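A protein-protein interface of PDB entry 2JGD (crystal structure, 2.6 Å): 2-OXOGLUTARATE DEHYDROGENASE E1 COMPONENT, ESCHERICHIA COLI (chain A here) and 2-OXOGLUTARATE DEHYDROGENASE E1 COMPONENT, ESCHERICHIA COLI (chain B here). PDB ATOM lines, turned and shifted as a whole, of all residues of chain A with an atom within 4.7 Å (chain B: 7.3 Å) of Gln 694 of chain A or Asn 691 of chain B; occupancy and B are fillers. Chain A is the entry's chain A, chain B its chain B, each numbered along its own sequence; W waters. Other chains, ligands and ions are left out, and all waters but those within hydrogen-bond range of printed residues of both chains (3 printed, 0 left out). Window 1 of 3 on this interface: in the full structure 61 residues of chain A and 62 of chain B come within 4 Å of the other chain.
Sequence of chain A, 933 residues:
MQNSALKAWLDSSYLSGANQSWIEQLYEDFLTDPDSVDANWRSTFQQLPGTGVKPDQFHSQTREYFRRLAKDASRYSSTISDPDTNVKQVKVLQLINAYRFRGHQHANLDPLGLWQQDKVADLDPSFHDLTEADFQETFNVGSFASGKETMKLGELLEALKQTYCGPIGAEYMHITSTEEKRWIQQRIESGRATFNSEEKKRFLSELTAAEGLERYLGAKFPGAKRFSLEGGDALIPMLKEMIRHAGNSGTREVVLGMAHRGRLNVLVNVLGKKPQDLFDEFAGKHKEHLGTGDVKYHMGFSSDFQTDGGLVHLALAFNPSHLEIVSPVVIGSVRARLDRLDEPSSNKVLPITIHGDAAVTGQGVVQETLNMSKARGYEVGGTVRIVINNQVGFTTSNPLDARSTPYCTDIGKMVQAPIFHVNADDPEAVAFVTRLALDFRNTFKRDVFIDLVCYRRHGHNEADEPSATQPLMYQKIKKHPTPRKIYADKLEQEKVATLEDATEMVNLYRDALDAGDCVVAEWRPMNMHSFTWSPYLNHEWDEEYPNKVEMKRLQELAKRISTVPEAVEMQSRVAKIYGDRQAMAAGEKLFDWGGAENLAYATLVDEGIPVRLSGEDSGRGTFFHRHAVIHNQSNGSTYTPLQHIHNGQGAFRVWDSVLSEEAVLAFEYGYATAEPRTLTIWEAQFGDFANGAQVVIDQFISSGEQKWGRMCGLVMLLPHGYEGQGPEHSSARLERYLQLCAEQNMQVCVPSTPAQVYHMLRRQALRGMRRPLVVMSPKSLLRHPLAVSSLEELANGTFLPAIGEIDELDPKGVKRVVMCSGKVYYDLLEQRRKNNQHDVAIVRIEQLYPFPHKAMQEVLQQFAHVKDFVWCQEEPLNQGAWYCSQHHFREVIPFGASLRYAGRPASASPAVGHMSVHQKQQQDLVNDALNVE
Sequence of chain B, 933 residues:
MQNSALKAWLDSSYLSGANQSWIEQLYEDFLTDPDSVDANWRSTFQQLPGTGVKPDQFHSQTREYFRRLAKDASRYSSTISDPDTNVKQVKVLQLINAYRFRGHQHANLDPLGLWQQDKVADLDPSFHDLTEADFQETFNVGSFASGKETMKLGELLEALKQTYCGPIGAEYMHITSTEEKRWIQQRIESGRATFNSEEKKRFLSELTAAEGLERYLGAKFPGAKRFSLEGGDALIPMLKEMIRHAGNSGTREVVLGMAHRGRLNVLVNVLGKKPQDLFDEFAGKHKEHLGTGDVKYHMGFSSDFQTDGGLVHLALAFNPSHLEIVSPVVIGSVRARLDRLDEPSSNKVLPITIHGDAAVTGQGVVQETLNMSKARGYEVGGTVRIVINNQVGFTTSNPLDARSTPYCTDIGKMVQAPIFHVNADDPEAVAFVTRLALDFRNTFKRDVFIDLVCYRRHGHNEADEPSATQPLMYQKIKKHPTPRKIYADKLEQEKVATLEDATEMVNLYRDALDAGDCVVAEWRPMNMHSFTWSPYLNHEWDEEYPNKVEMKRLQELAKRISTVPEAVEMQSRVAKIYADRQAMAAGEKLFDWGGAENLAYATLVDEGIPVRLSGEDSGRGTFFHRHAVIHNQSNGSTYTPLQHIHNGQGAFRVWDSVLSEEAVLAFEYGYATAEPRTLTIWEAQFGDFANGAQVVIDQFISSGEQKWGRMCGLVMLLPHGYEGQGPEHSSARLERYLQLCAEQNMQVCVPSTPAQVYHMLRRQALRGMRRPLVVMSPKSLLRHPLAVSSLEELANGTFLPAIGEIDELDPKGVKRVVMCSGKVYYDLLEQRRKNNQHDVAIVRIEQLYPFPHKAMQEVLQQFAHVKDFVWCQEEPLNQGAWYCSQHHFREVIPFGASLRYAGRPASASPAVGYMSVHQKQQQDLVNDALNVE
CE1 of His 322 of chain A touches O of Asp 688 of chain B, at 3.4 Å.
His 322 of chain A touches Phe 689 of chain B.
CE1 of His 322 of chain A touches OD1 of Asn 691 of chain B, at 2.9 Å.
Asn 691 of chain A touches Val 695 of chain B (OD1 to CG2, 3.7 Å).
Val 695 of chain B touches Gly 692 of chain A (CG2 to CA, 3.8 Å).
Asn 691 of chain B touches Gln 694 of chain A (O to CB, 3.8 Å).
CG of Gln 694 of chain A touches CG of Gln 694 of chain B (3.5 Å).
Gln 694 of chain A touches Arg 736 of chain B (CG to NH1, 3.5 Å).
Val 695 of chain A touches Asn 691 of chain B (CG2 to OD1, 3.8 Å).
CG2 of Val 695 of chain A touches CA of Gly 692 of chain B, 3.6 Å away.
Of chain B, only Asn 691, Gln 694 and Arg 736 come within 4 Å of Gln 694 of chain A.
Asn 691 of chain B touches just these residues of chain A: His 322, Gln 694, Val 695, Asp 698 and Gln 699.
Of the printed residues of chain A, Asp 688 of chain B touches His 322 (3.4 Å).
Printed residues of chain A within 4 Å of Arg 733 of chain B: Asp 698 and Gln 699.
Gly 687 of chain B touches none of the printed residues of chain A.
The nearest printed residue of chain A that does not touch Asn 691 of chain B is Asn 691 of chain A (5.3 Å).
The side-chain carboxylate (OD2) of Asp 698 of chain A lies within salt-bridge range of the guanidinium group (NE) of Arg 733 of chain B, 3.97 Å away.
The side-chain amide oxygen (OE1) of Gln 699 of chain A sits at hydrogen-bond distance from the side-chain amide nitrogen (ND2) of Asn 691 of chain B, at 2.9 Å.
OD2 of Asp 698 of chain A is in salt-bridge range of NH1 of Arg 736 of chain B, at 2.8 Å.
OD2 of Asp 698 of chain A is in hydrogen-bond range of ND2 of Asn 691 of chain B (2.9 Å).
NE2 of Gln 694 of chain B lies close to NH2 of Arg 736 of chain A (3.5 Å).
The guanidinium group of Arg 736 of chain B lies close to the guanidinium group of Arg 736 of chain A, at 3.5 Å.
The guanidinium group (NH1) of Arg 736 of chain A is in salt-bridge range of the side-chain carboxylate (OD2) of Asp 698 of chain B (2.7 Å).
The side-chain amide nitrogen (ND2) of Asn 691 of chain A sits at hydrogen-bond distance from the side-chain carboxylate (OD2) of Asp 698 of chain B (2.8 Å).
The side-chain amide oxygen (OD1) of Asn 691 of chain B lies close to the backbone carbonyl oxygen (O) of Phe 689 of chain B (3.3 Å).
The guanidinium group of Arg 736 of chain B lies within hydrogen-bond range of the side-chain amide oxygen of Gln 694 of chain B.
The backbone carbonyl oxygen (O) of Val 695 of chain A sits close to the side-chain amide oxygen (OE1) of Gln 699 of chain A, at 3.3 Å.
OD1 of Asn 691 of chain B lies close to O of Asp 688 of chain B, at 3.2 Å.
The side-chain amide oxygen (OE1) of Gln 699 of chain A sits close to a ring nitrogen (NE2) of His 322 of chain A, at 3.4 Å.
NE2 of Gln 694 of chain A sits at hydrogen-bond distance from OD1 of Asp 698 of chain A (2.8 Å).
Water W2 lies within hydrogen-bond range of O of Asp 688 of chain B (2.7 Å), NE of Arg 733 of chain B (2.9 Å) and NE2 of Gln 699 of chain A (3.1 Å).
Water W3 bridges the backbone carbonyl oxygen of Asn 691 of chain A and the backbone carbonyl oxygen of Asn 691 of chain B.
Water W1 lies within hydrogen-bond range of the guanidinium group of Arg 733 of chain B (3.3 Å) and the backbone carbonyl oxygen of Asp 698 of chain A (3.4 Å).
Hydrophobic or aromatic side chains of chain A that line the printed part of chain B: His 322 and Val 695.
Along chain B the printed residues that touch a printed residue of chain A span positions 688 to 736.
Among the printed residues, 20 pairs touch across the chains.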
ATOM      1  N   HIS A 322       6.838   2.562  10.287  1.00  0.00           N
ATOM      2  CA  HIS A 322       6.662   1.275  10.951  1.00  0.00           C
ATOM      3  C   HIS A 322       7.563   0.210  10.335  1.00  0.00           C
ATOM      4  O   HIS A 322       7.476  -0.075   9.141  1.00  0.00           O
ATOM      5  CB  HIS A 322       5.199   0.832  10.881  1.00  0.00           C
ATOM      6  CG  HIS A 322       4.235   1.843  11.418  1.00  0.00           C
ATOM      7  ND1 HIS A 322       3.381   1.574  12.466  1.00  0.00           N
ATOM      8  CD2 HIS A 322       3.989   3.123  11.052  1.00  0.00           C
ATOM      9  CE1 HIS A 322       2.651   2.644  12.722  1.00  0.00           C
ATOM     10  NE2 HIS A 322       3.000   3.598  11.878  1.00  0.00           N
ATOM     11  N   ALA A 690     -10.002  -7.658  12.375  1.00  0.00           N
ATOM     12  CA  ALA A 690      -9.162  -7.010  11.380  1.00  0.00           C
ATOM     13  C   ALA A 690      -8.206  -6.011  12.024  1.00  0.00           C
ATOM     14  O   ALA A 690      -7.149  -5.693  11.461  1.00  0.00           O
ATOM     15  CB  ALA A 690      -9.988  -6.368  10.309  1.00  0.00           C
ATOM     16  N   ASN A 691      -8.532  -5.574  13.234  1.00  0.00           N
ATOM     17  CA  ASN A 691      -7.639  -4.668  13.949  1.00  0.00           C
ATOM     18  C   ASN A 691      -6.298  -5.304  14.249  1.00  0.00           C
ATOM     19  O   ASN A 691      -5.321  -4.608  14.548  1.00  0.00           O
ATOM     20  CB  ASN A 691      -8.283  -4.080  15.207  1.00  0.00           C
ATOM     21  CG  ASN A 691      -8.652  -5.126  16.224  1.00  0.00           C
ATOM     22  OD1 ASN A 691      -8.467  -6.316  16.000  1.00  0.00           O
ATOM     23  ND2 ASN A 691      -9.182  -4.685  17.364  1.00  0.00           N
ATOM     24  N   GLY A 692      -6.224  -6.625  14.118  1.00  0.00           N
ATOM     25  CA  GLY A 692      -4.924  -7.282  14.143  1.00  0.00           C
ATOM     26  C   GLY A 692      -4.025  -6.789  13.018  1.00  0.00           C
ATOM     27  O   GLY A 692      -2.842  -7.103  12.995  1.00  0.00           O
ATOM     28  N   ALA A 693      -4.599  -6.035  12.073  1.00  0.00           N
ATOM     29  CA  ALA A 693      -3.868  -5.581  10.887  1.00  0.00           C
ATOM     30  C   ALA A 693      -3.949  -4.059  10.745  1.00  0.00           C
ATOM     31  O   ALA A 693      -3.801  -3.508   9.653  1.00  0.00           O
ATOM     32  CB  ALA A 693      -4.407  -6.256   9.635  1.00  0.00           C
ATOM     33  N   GLN A 694      -4.204  -3.390  11.860  1.00  0.00           N
ATOM     34  CA  GLN A 694      -4.408  -1.958  11.866  1.00  0.00           C
ATOM     35  C   GLN A 694      -3.304  -1.229  11.116  1.00  0.00           C
ATOM     36  O   GLN A 694      -3.573  -0.274  10.374  1.00  0.00           O
ATOM     37  CB  GLN A 694      -4.495  -1.430  13.299  1.00  0.00           C
ATOM     38  CG  GLN A 694      -5.297  -0.157  13.406  1.00  0.00           C
ATOM     39  CD  GLN A 694      -6.707  -0.324  12.867  1.00  0.00           C
ATOM     40  OE1 GLN A 694      -7.459  -1.160  13.334  1.00  0.00           O
ATOM     41  NE2 GLN A 694      -7.063   0.480  11.887  1.00  0.00           N
ATOM     42  N   VAL A 695      -2.056  -1.640  11.320  1.00  0.00           N
ATOM     43  CA  VAL A 695      -0.964  -0.934  10.670  1.00  0.00           C
ATOM     44  C   VAL A 695      -1.122  -0.963   9.142  1.00  0.00           C
ATOM     45  O   VAL A 695      -0.934   0.048   8.462  1.00  0.00           O
ATOM     46  CB  VAL A 695       0.404  -1.461  11.096  1.00  0.00           C
ATOM     47  CG1 VAL A 695       1.490  -0.818  10.262  1.00  0.00           C
ATOM     48  CG2 VAL A 695       0.641  -1.147  12.560  1.00  0.00           C
ATOM     49  N   VAL A 696      -1.530  -2.104   8.608  1.00  0.00           N
ATOM     50  CA  VAL A 696      -1.764  -2.183   7.190  1.00  0.00           C
ATOM     51  C   VAL A 696      -2.896  -1.286   6.772  1.00  0.00           C
ATOM     52  O   VAL A 696      -2.816  -0.584   5.758  1.00  0.00           O
ATOM     53  CB  VAL A 696      -2.089  -3.581   6.728  1.00  0.00           C
ATOM     54  CG1 VAL A 696      -2.218  -3.572   5.232  1.00  0.00           C
ATOM     55  CG2 VAL A 696      -1.007  -4.556   7.173  1.00  0.00           C
ATOM     56  N   ILE A 697      -3.981  -1.335   7.522  1.00  0.00           N
ATOM     57  CA  ILE A 697      -5.116  -0.495   7.185  1.00  0.00           C
ATOM     58  C   ILE A 697      -4.733   0.987   7.245  1.00  0.00           C
ATOM     59  O   ILE A 697      -5.144   1.792   6.397  1.00  0.00           O
ATOM     60  CB  ILE A 697      -6.288  -0.768   8.095  1.00  0.00           C
ATOM     61  CG1 ILE A 697      -6.847  -2.168   7.810  1.00  0.00           C
ATOM     62  CG2 ILE A 697      -7.352   0.365   7.986  1.00  0.00           C
ATOM     63  CD1 ILE A 697      -7.797  -2.693   8.947  1.00  0.00           C
ATOM     64  N   ASP A 698      -3.936   1.345   8.239  1.00  0.00           N
ATOM     65  CA  ASP A 698      -3.692   2.754   8.535  1.00  0.00           C
ATOM     66  C   ASP A 698      -2.591   3.296   7.634  1.00  0.00           C
ATOM     67  O   ASP A 698      -2.726   4.384   7.092  1.00  0.00           O
ATOM     68  CB  ASP A 698      -3.272   2.937   9.996  1.00  0.00           C
ATOM     69  CG  ASP A 698      -4.410   2.671  10.990  1.00  0.00           C
ATOM     70  OD1 ASP A 698      -5.569   2.466  10.570  1.00  0.00           O
ATOM     71  OD2 ASP A 698      -4.136   2.675  12.211  1.00  0.00           O
ATOM     72  N   GLN A 699      -1.490   2.551   7.502  1.00  0.00           N
ATOM     73  CA  GLN A 699      -0.287   3.069   6.845  1.00  0.00           C
ATOM     74  C   GLN A 699      -0.219   2.809   5.331  1.00  0.00           C
ATOM     75  O   GLN A 699       0.606   3.388   4.648  1.00  0.00           O
ATOM     76  CB  GLN A 699       0.989   2.540   7.509  1.00  0.00           C
ATOM     77  CG  GLN A 699       1.543   3.465   8.581  1.00  0.00           C
ATOM     78  CD  GLN A 699       0.598   3.571   9.748  1.00  0.00           C
ATOM     79  OE1 GLN A 699       0.165   2.563  10.299  1.00  0.00           O
ATOM     80  NE2 GLN A 699       0.234   4.786  10.102  1.00  0.00           N
ATOM     81  N   ARG A 736     -14.449   3.207  12.419  1.00  0.00           N
ATOM     82  CA  ARG A 736     -13.014   3.418  12.245  1.00  0.00           C
ATOM     83  C   ARG A 736     -12.633   3.592  10.777  1.00  0.00           C
ATOM     84  O   ARG A 736     -11.793   4.417  10.438  1.00  0.00           O
ATOM     85  CB  ARG A 736     -12.206   2.306  12.872  1.00  0.00           C
ATOM     86  CG  ARG A 736     -10.718   2.595  12.823  1.00  0.00           C
ATOM     87  CD  ARG A 736      -9.906   1.692  13.737  1.00  0.00           C
ATOM     88  NE  ARG A 736     -10.265   1.796  15.154  1.00  0.00           N
ATOM     89  CZ  ARG A 736      -9.944   0.875  16.065  1.00  0.00           C
ATOM     90  NH1 ARG A 736      -9.253  -0.206  15.716  1.00  0.00           N
ATOM     91  NH2 ARG A 736     -10.315   1.024  17.322  1.00  0.00           N
ATOM     92  N   GLU B 661       6.307  -3.504  20.262  1.00  0.00           N
ATOM     93  CA  GLU B 661       5.343  -2.601  20.851  1.00  0.00           C
ATOM     94  C   GLU B 661       4.065  -3.278  21.357  1.00  0.00           C
ATOM     95  O   GLU B 661       3.528  -2.905  22.402  1.00  0.00           O
ATOM     96  CB  GLU B 661       4.990  -1.481  19.864  1.00  0.00           C
ATOM     97  CG  GLU B 661       4.630  -0.188  20.559  1.00  0.00           C
ATOM     98  CD  GLU B 661       4.080   0.832  19.625  1.00  0.00           C
ATOM     99  OE1 GLU B 661       3.188   0.476  18.823  1.00  0.00           O
ATOM    100  OE2 GLU B 661       4.531   1.992  19.689  1.00  0.00           O
ATOM    101  N   GLU B 662       3.533  -4.220  20.587  1.00  0.00           N
ATOM    102  CA  GLU B 662       2.294  -4.868  20.972  1.00  0.00           C
ATOM    103  C   GLU B 662       2.473  -5.641  22.310  1.00  0.00           C
ATOM    104  O   GLU B 662       1.619  -5.586  23.175  1.00  0.00           O
ATOM    105  CB  GLU B 662       1.821  -5.785  19.845  1.00  0.00           C
ATOM    106  CG  GLU B 662       0.441  -6.431  20.053  1.00  0.00           C
ATOM    107  CD  GLU B 662       0.162  -7.529  19.025  1.00  0.00           C
ATOM    108  OE1 GLU B 662       1.142  -8.066  18.449  1.00  0.00           O
ATOM    109  OE2 GLU B 662      -1.023  -7.846  18.780  1.00  0.00           O
ATOM    110  N   TRP B 682       3.312   3.904  30.257  1.00  0.00           N
ATOM    111  CA  TRP B 682       3.902   3.548  28.959  1.00  0.00           C
ATOM    112  C   TRP B 682       3.986   4.708  27.971  1.00  0.00           C
ATOM    113  O   TRP B 682       3.005   5.412  27.727  1.00  0.00           O
ATOM    114  CB  TRP B 682       3.169   2.371  28.302  1.00  0.00           C
ATOM    115  CG  TRP B 682       3.778   1.945  26.960  1.00  0.00           C
ATOM    116  CD1 TRP B 682       4.888   1.181  26.781  1.00  0.00           C
ATOM    117  CD2 TRP B 682       3.291   2.257  25.636  1.00  0.00           C
ATOM    118  NE1 TRP B 682       5.136   1.004  25.437  1.00  0.00           N
ATOM    119  CE2 TRP B 682       4.179   1.659  24.714  1.00  0.00           C
ATOM    120  CE3 TRP B 682       2.195   2.975  25.148  1.00  0.00           C
ATOM    121  CZ2 TRP B 682       4.017   1.768  23.333  1.00  0.00           C
ATOM    122  CZ3 TRP B 682       2.022   3.078  23.765  1.00  0.00           C
ATOM    123  CH2 TRP B 682       2.928   2.474  22.873  1.00  0.00           C
ATOM    124  N   PHE B 686       6.691   7.691  19.127  1.00  0.00           N
ATOM    125  CA  PHE B 686       5.688   8.658  18.689  1.00  0.00           C
ATOM    126  C   PHE B 686       4.319   8.032  18.742  1.00  0.00           C
ATOM    127  O   PHE B 686       4.170   6.837  18.499  1.00  0.00           O
ATOM    128  CB  PHE B 686       5.934   9.057  17.236  1.00  0.00           C
ATOM    129  CG  PHE B 686       7.159   9.852  17.040  1.00  0.00           C
ATOM    130  CD1 PHE B 686       8.392   9.245  17.075  1.00  0.00           C
ATOM    131  CD2 PHE B 686       7.081  11.208  16.803  1.00  0.00           C
ATOM    132  CE1 PHE B 686       9.532   9.981  16.889  1.00  0.00           C
ATOM    133  CE2 PHE B 686       8.209  11.951  16.634  1.00  0.00           C
ATOM    134  CZ  PHE B 686       9.440  11.348  16.687  1.00  0.00           C
ATOM    135  N   GLY B 687       3.301   8.850  18.963  1.00  0.00           N
ATOM    136  CA  GLY B 687       1.954   8.320  19.105  1.00  0.00           C
ATOM    137  C   GLY B 687       1.508   7.530  17.892  1.00  0.00           C
ATOM    138  O   GLY B 687       0.704   6.595  18.002  1.00  0.00           O
ATOM    139  N   ASP B 688       2.047   7.910  16.741  1.00  0.00           N
ATOM    140  CA  ASP B 688       1.697   7.326  15.449  1.00  0.00           C
ATOM    141  C   ASP B 688       1.936   5.828  15.418  1.00  0.00           C
ATOM    142  O   ASP B 688       1.339   5.120  14.624  1.00  0.00           O
ATOM    143  CB  ASP B 688       2.539   7.992  14.349  1.00  0.00           C
ATOM    144  CG  ASP B 688       2.631   9.531  14.511  1.00  0.00           C
ATOM    145  OD1 ASP B 688       2.135  10.265  13.624  1.00  0.00           O
ATOM    146  OD2 ASP B 688       3.186  10.004  15.532  1.00  0.00           O
ATOM    147  N   PHE B 689       2.823   5.340  16.271  1.00  0.00           N
ATOM    148  CA  PHE B 689       3.174   3.930  16.226  1.00  0.00           C
ATOM    149  C   PHE B 689       2.279   3.043  17.096  1.00  0.00           C
ATOM    150  O   PHE B 689       2.263   1.816  16.944  1.00  0.00           O
ATOM    151  CB  PHE B 689       4.630   3.736  16.611  1.00  0.00           C
ATOM    152  CG  PHE B 689       5.591   4.380  15.661  1.00  0.00           C
ATOM    153  CD1 PHE B 689       6.481   5.323  16.097  1.00  0.00           C
ATOM    154  CD2 PHE B 689       5.573   4.063  14.316  1.00  0.00           C
ATOM    155  CE1 PHE B 689       7.331   5.946  15.218  1.00  0.00           C
ATOM    156  CE2 PHE B 689       6.444   4.667  13.438  1.00  0.00           C
ATOM    157  CZ  PHE B 689       7.317   5.616  13.895  1.00  0.00           C
ATOM    158  N   ALA B 690       1.558   3.651  18.028  1.00  0.00           N
ATOM    159  CA  ALA B 690       0.807   2.868  18.972  1.00  0.00           C
ATOM    160  C   ALA B 690      -0.214   1.998  18.292  1.00  0.00           C
ATOM    161  O   ALA B 690      -0.696   1.036  18.883  1.00  0.00           O
ATOM    162  CB  ALA B 690       0.142   3.732  19.985  1.00  0.00           C
ATOM    163  N   ASN B 691      -0.561   2.310  17.052  1.00  0.00           N
ATOM    164  CA  ASN B 691      -1.528   1.450  16.361  1.00  0.00           C
ATOM    165  C   ASN B 691      -0.998   0.055  16.115  1.00  0.00           C
ATOM    166  O   ASN B 691      -1.761  -0.872  15.934  1.00  0.00           O
ATOM    167  CB  ASN B 691      -2.029   2.061  15.065  1.00  0.00           C
ATOM    168  CG  ASN B 691      -0.933   2.232  14.046  1.00  0.00           C
ATOM    169  OD1 ASN B 691       0.261   2.133  14.357  1.00  0.00           O
ATOM    170  ND2 ASN B 691      -1.328   2.508  12.822  1.00  0.00           N
ATOM    171  N   GLY B 692       0.324  -0.082  16.108  1.00  0.00           N
ATOM    172  CA  GLY B 692       0.955  -1.386  16.181  1.00  0.00           C
ATOM    173  C   GLY B 692       0.380  -2.249  17.284  1.00  0.00           C
ATOM    174  O   GLY B 692       0.531  -3.470  17.273  1.00  0.00           O
ATOM    175  N   ALA B 693      -0.283  -1.610  18.242  1.00  0.00           N
ATOM    176  CA  ALA B 693      -0.792  -2.306  19.418  1.00  0.00           C
ATOM    177  C   ALA B 693      -2.304  -2.156  19.537  1.00  0.00           C
ATOM    178  O   ALA B 693      -2.852  -2.156  20.640  1.00  0.00           O
ATOM    179  CB  ALA B 693      -0.104  -1.797  20.675  1.00  0.00           C
ATOM    180  N   GLN B 694      -2.973  -2.026  18.397  1.00  0.00           N
ATOM    181  CA  GLN B 694      -4.389  -1.675  18.374  1.00  0.00           C
ATOM    182  C   GLN B 694      -5.222  -2.691  19.147  1.00  0.00           C
ATOM    183  O   GLN B 694      -6.224  -2.342  19.771  1.00  0.00           O
ATOM    184  CB  GLN B 694      -4.891  -1.570  16.933  1.00  0.00           C
ATOM    185  CG  GLN B 694      -6.182  -0.780  16.782  1.00  0.00           C
ATOM    186  CD  GLN B 694      -6.086   0.612  17.374  1.00  0.00           C
ATOM    187  OE1 GLN B 694      -5.220   1.398  16.987  1.00  0.00           O
ATOM    188  NE2 GLN B 694      -6.973   0.922  18.312  1.00  0.00           N
ATOM    189  N   VAL B 695      -4.801  -3.951  19.101  1.00  0.00           N
ATOM    190  CA  VAL B 695      -5.568  -5.038  19.698  1.00  0.00           C
ATOM    191  C   VAL B 695      -5.613  -4.911  21.218  1.00  0.00           C
ATOM    192  O   VAL B 695      -6.657  -5.114  21.837  1.00  0.00           O
ATOM    193  CB  VAL B 695      -4.984  -6.413  19.324  1.00  0.00           C
ATOM    194  CG1 VAL B 695      -5.500  -7.486  20.272  1.00  0.00           C
ATOM    195  CG2 VAL B 695      -5.319  -6.760  17.882  1.00  0.00           C
ATOM    196  N   ILE B 697      -5.301  -2.078  22.792  1.00  0.00           N
ATOM    197  CA  ILE B 697      -6.139  -0.907  23.023  1.00  0.00           C
ATOM    198  C   ILE B 697      -7.619  -1.260  22.922  1.00  0.00           C
ATOM    199  O   ILE B 697      -8.419  -0.872  23.774  1.00  0.00           O
ATOM    200  CB  ILE B 697      -5.792   0.210  22.021  1.00  0.00           C
ATOM    201  CG1 ILE B 697      -4.432   0.825  22.358  1.00  0.00           C
ATOM    202  CG2 ILE B 697      -6.878   1.276  22.015  1.00  0.00           C
ATOM    203  CD1 ILE B 697      -3.760   1.503  21.184  1.00  0.00           C
ATOM    204  N   ASP B 698      -7.978  -1.997  21.875  1.00  0.00           N
ATOM    205  CA  ASP B 698      -9.378  -2.236  21.550  1.00  0.00           C
ATOM    206  C   ASP B 698     -10.011  -3.223  22.526  1.00  0.00           C
ATOM    207  O   ASP B 698     -11.161  -3.058  22.931  1.00  0.00           O
ATOM    208  CB  ASP B 698      -9.514  -2.754  20.117  1.00  0.00           C
ATOM    209  CG  ASP B 698      -9.249  -1.679  19.082  1.00  0.00           C
ATOM    210  OD1 ASP B 698      -9.111  -0.500  19.469  1.00  0.00           O
ATOM    211  OD2 ASP B 698      -9.163  -1.918  17.859  1.00  0.00           O
ATOM    212  N   ALA B 732      -1.077  11.180  16.973  1.00  0.00           N
ATOM    213  CA  ALA B 732      -1.377   9.986  17.784  1.00  0.00           C
ATOM    214  C   ALA B 732      -2.759   9.390  17.473  1.00  0.00           C
ATOM    215  O   ALA B 732      -3.160   8.405  18.069  1.00  0.00           O
ATOM    216  CB  ALA B 732      -1.236  10.271  19.265  1.00  0.00           C
ATOM    217  N   ARG B 733      -3.482  10.004  16.538  1.00  0.00           N
ATOM    218  CA  ARG B 733      -4.847   9.582  16.229  1.00  0.00           C
ATOM    219  C   ARG B 733      -5.797   9.799  17.424  1.00  0.00           C
ATOM    220  O   ARG B 733      -6.578   8.922  17.805  1.00  0.00           O
ATOM    221  CB  ARG B 733      -4.872   8.132  15.699  1.00  0.00           C
ATOM    222  CG  ARG B 733      -3.989   7.944  14.477  1.00  0.00           C
ATOM    223  CD  ARG B 733      -4.273   6.664  13.709  1.00  0.00           C
ATOM    224  NE  ARG B 733      -3.361   6.554  12.579  1.00  0.00           N
ATOM    225  CZ  ARG B 733      -3.684   6.781  11.308  1.00  0.00           C
ATOM    226  NH1 ARG B 733      -2.755   6.677  10.370  1.00  0.00           N
ATOM    227  NH2 ARG B 733      -4.931   7.056  10.959  1.00  0.00           N
ATOM    228  N   ARG B 736      -9.224   8.508  17.273  1.00  0.00           N
ATOM    229  CA  ARG B 736      -9.513   7.110  17.512  1.00  0.00           C
ATOM    230  C   ARG B 736      -9.694   6.770  18.990  1.00  0.00           C
ATOM    231  O   ARG B 736     -10.541   5.974  19.359  1.00  0.00           O
ATOM    232  CB  ARG B 736      -8.440   6.243  16.903  1.00  0.00           C
ATOM    233  CG  ARG B 736      -8.769   4.790  16.949  1.00  0.00           C
ATOM    234  CD  ARG B 736      -7.730   4.012  16.202  1.00  0.00           C
ATOM    235  NE  ARG B 736      -7.802   4.216  14.761  1.00  0.00           N
ATOM    236  CZ  ARG B 736      -6.860   3.790  13.943  1.00  0.00           C
ATOM    237  NH1 ARG B 736      -5.802   3.173  14.453  1.00  0.00           N
ATOM    238  NH2 ARG B 736      -6.956   3.985  12.634  1.00  0.00           N
ATOM    239  N   TYR B 737      -8.910   7.392  19.846  1.00  0.00           N
ATOM    240  CA  TYR B 737      -9.176   7.280  21.260  1.00  0.00           C
ATOM    241  C   TYR B 737     -10.494   7.939  21.644  1.00  0.00           C
ATOM    242  O   TYR B 737     -11.233   7.418  22.479  1.00  0.00           O
ATOM    243  CB  TYR B 737      -8.026   7.851  22.065  1.00  0.00           C
ATOM    244  CG  TYR B 737      -6.736   7.099  21.841  1.00  0.00           C
ATOM    245  CD1 TYR B 737      -5.802   7.560  20.933  1.00  0.00           C
ATOM    246  CD2 TYR B 737      -6.489   5.879  22.486  1.00  0.00           C
ATOM    247  CE1 TYR B 737      -4.634   6.858  20.691  1.00  0.00           C
ATOM    248  CE2 TYR B 737      -5.321   5.175  22.253  1.00  0.00           C
ATOM    249  CZ  TYR B 737      -4.397   5.678  21.355  1.00  0.00           C
ATOM    250  OH  TYR B 737      -3.241   5.012  21.106  1.00  0.00           O
HETATM  251  O   HOH W   1      -4.470   7.310   7.592  1.00  0.00           O
HETATM  252  O   HOH W   2      -0.469   6.060  12.819  1.00  0.00           O
HETATM  253  O   HOH W   3      -2.502  -4.054  15.296  1.00  0.00           O
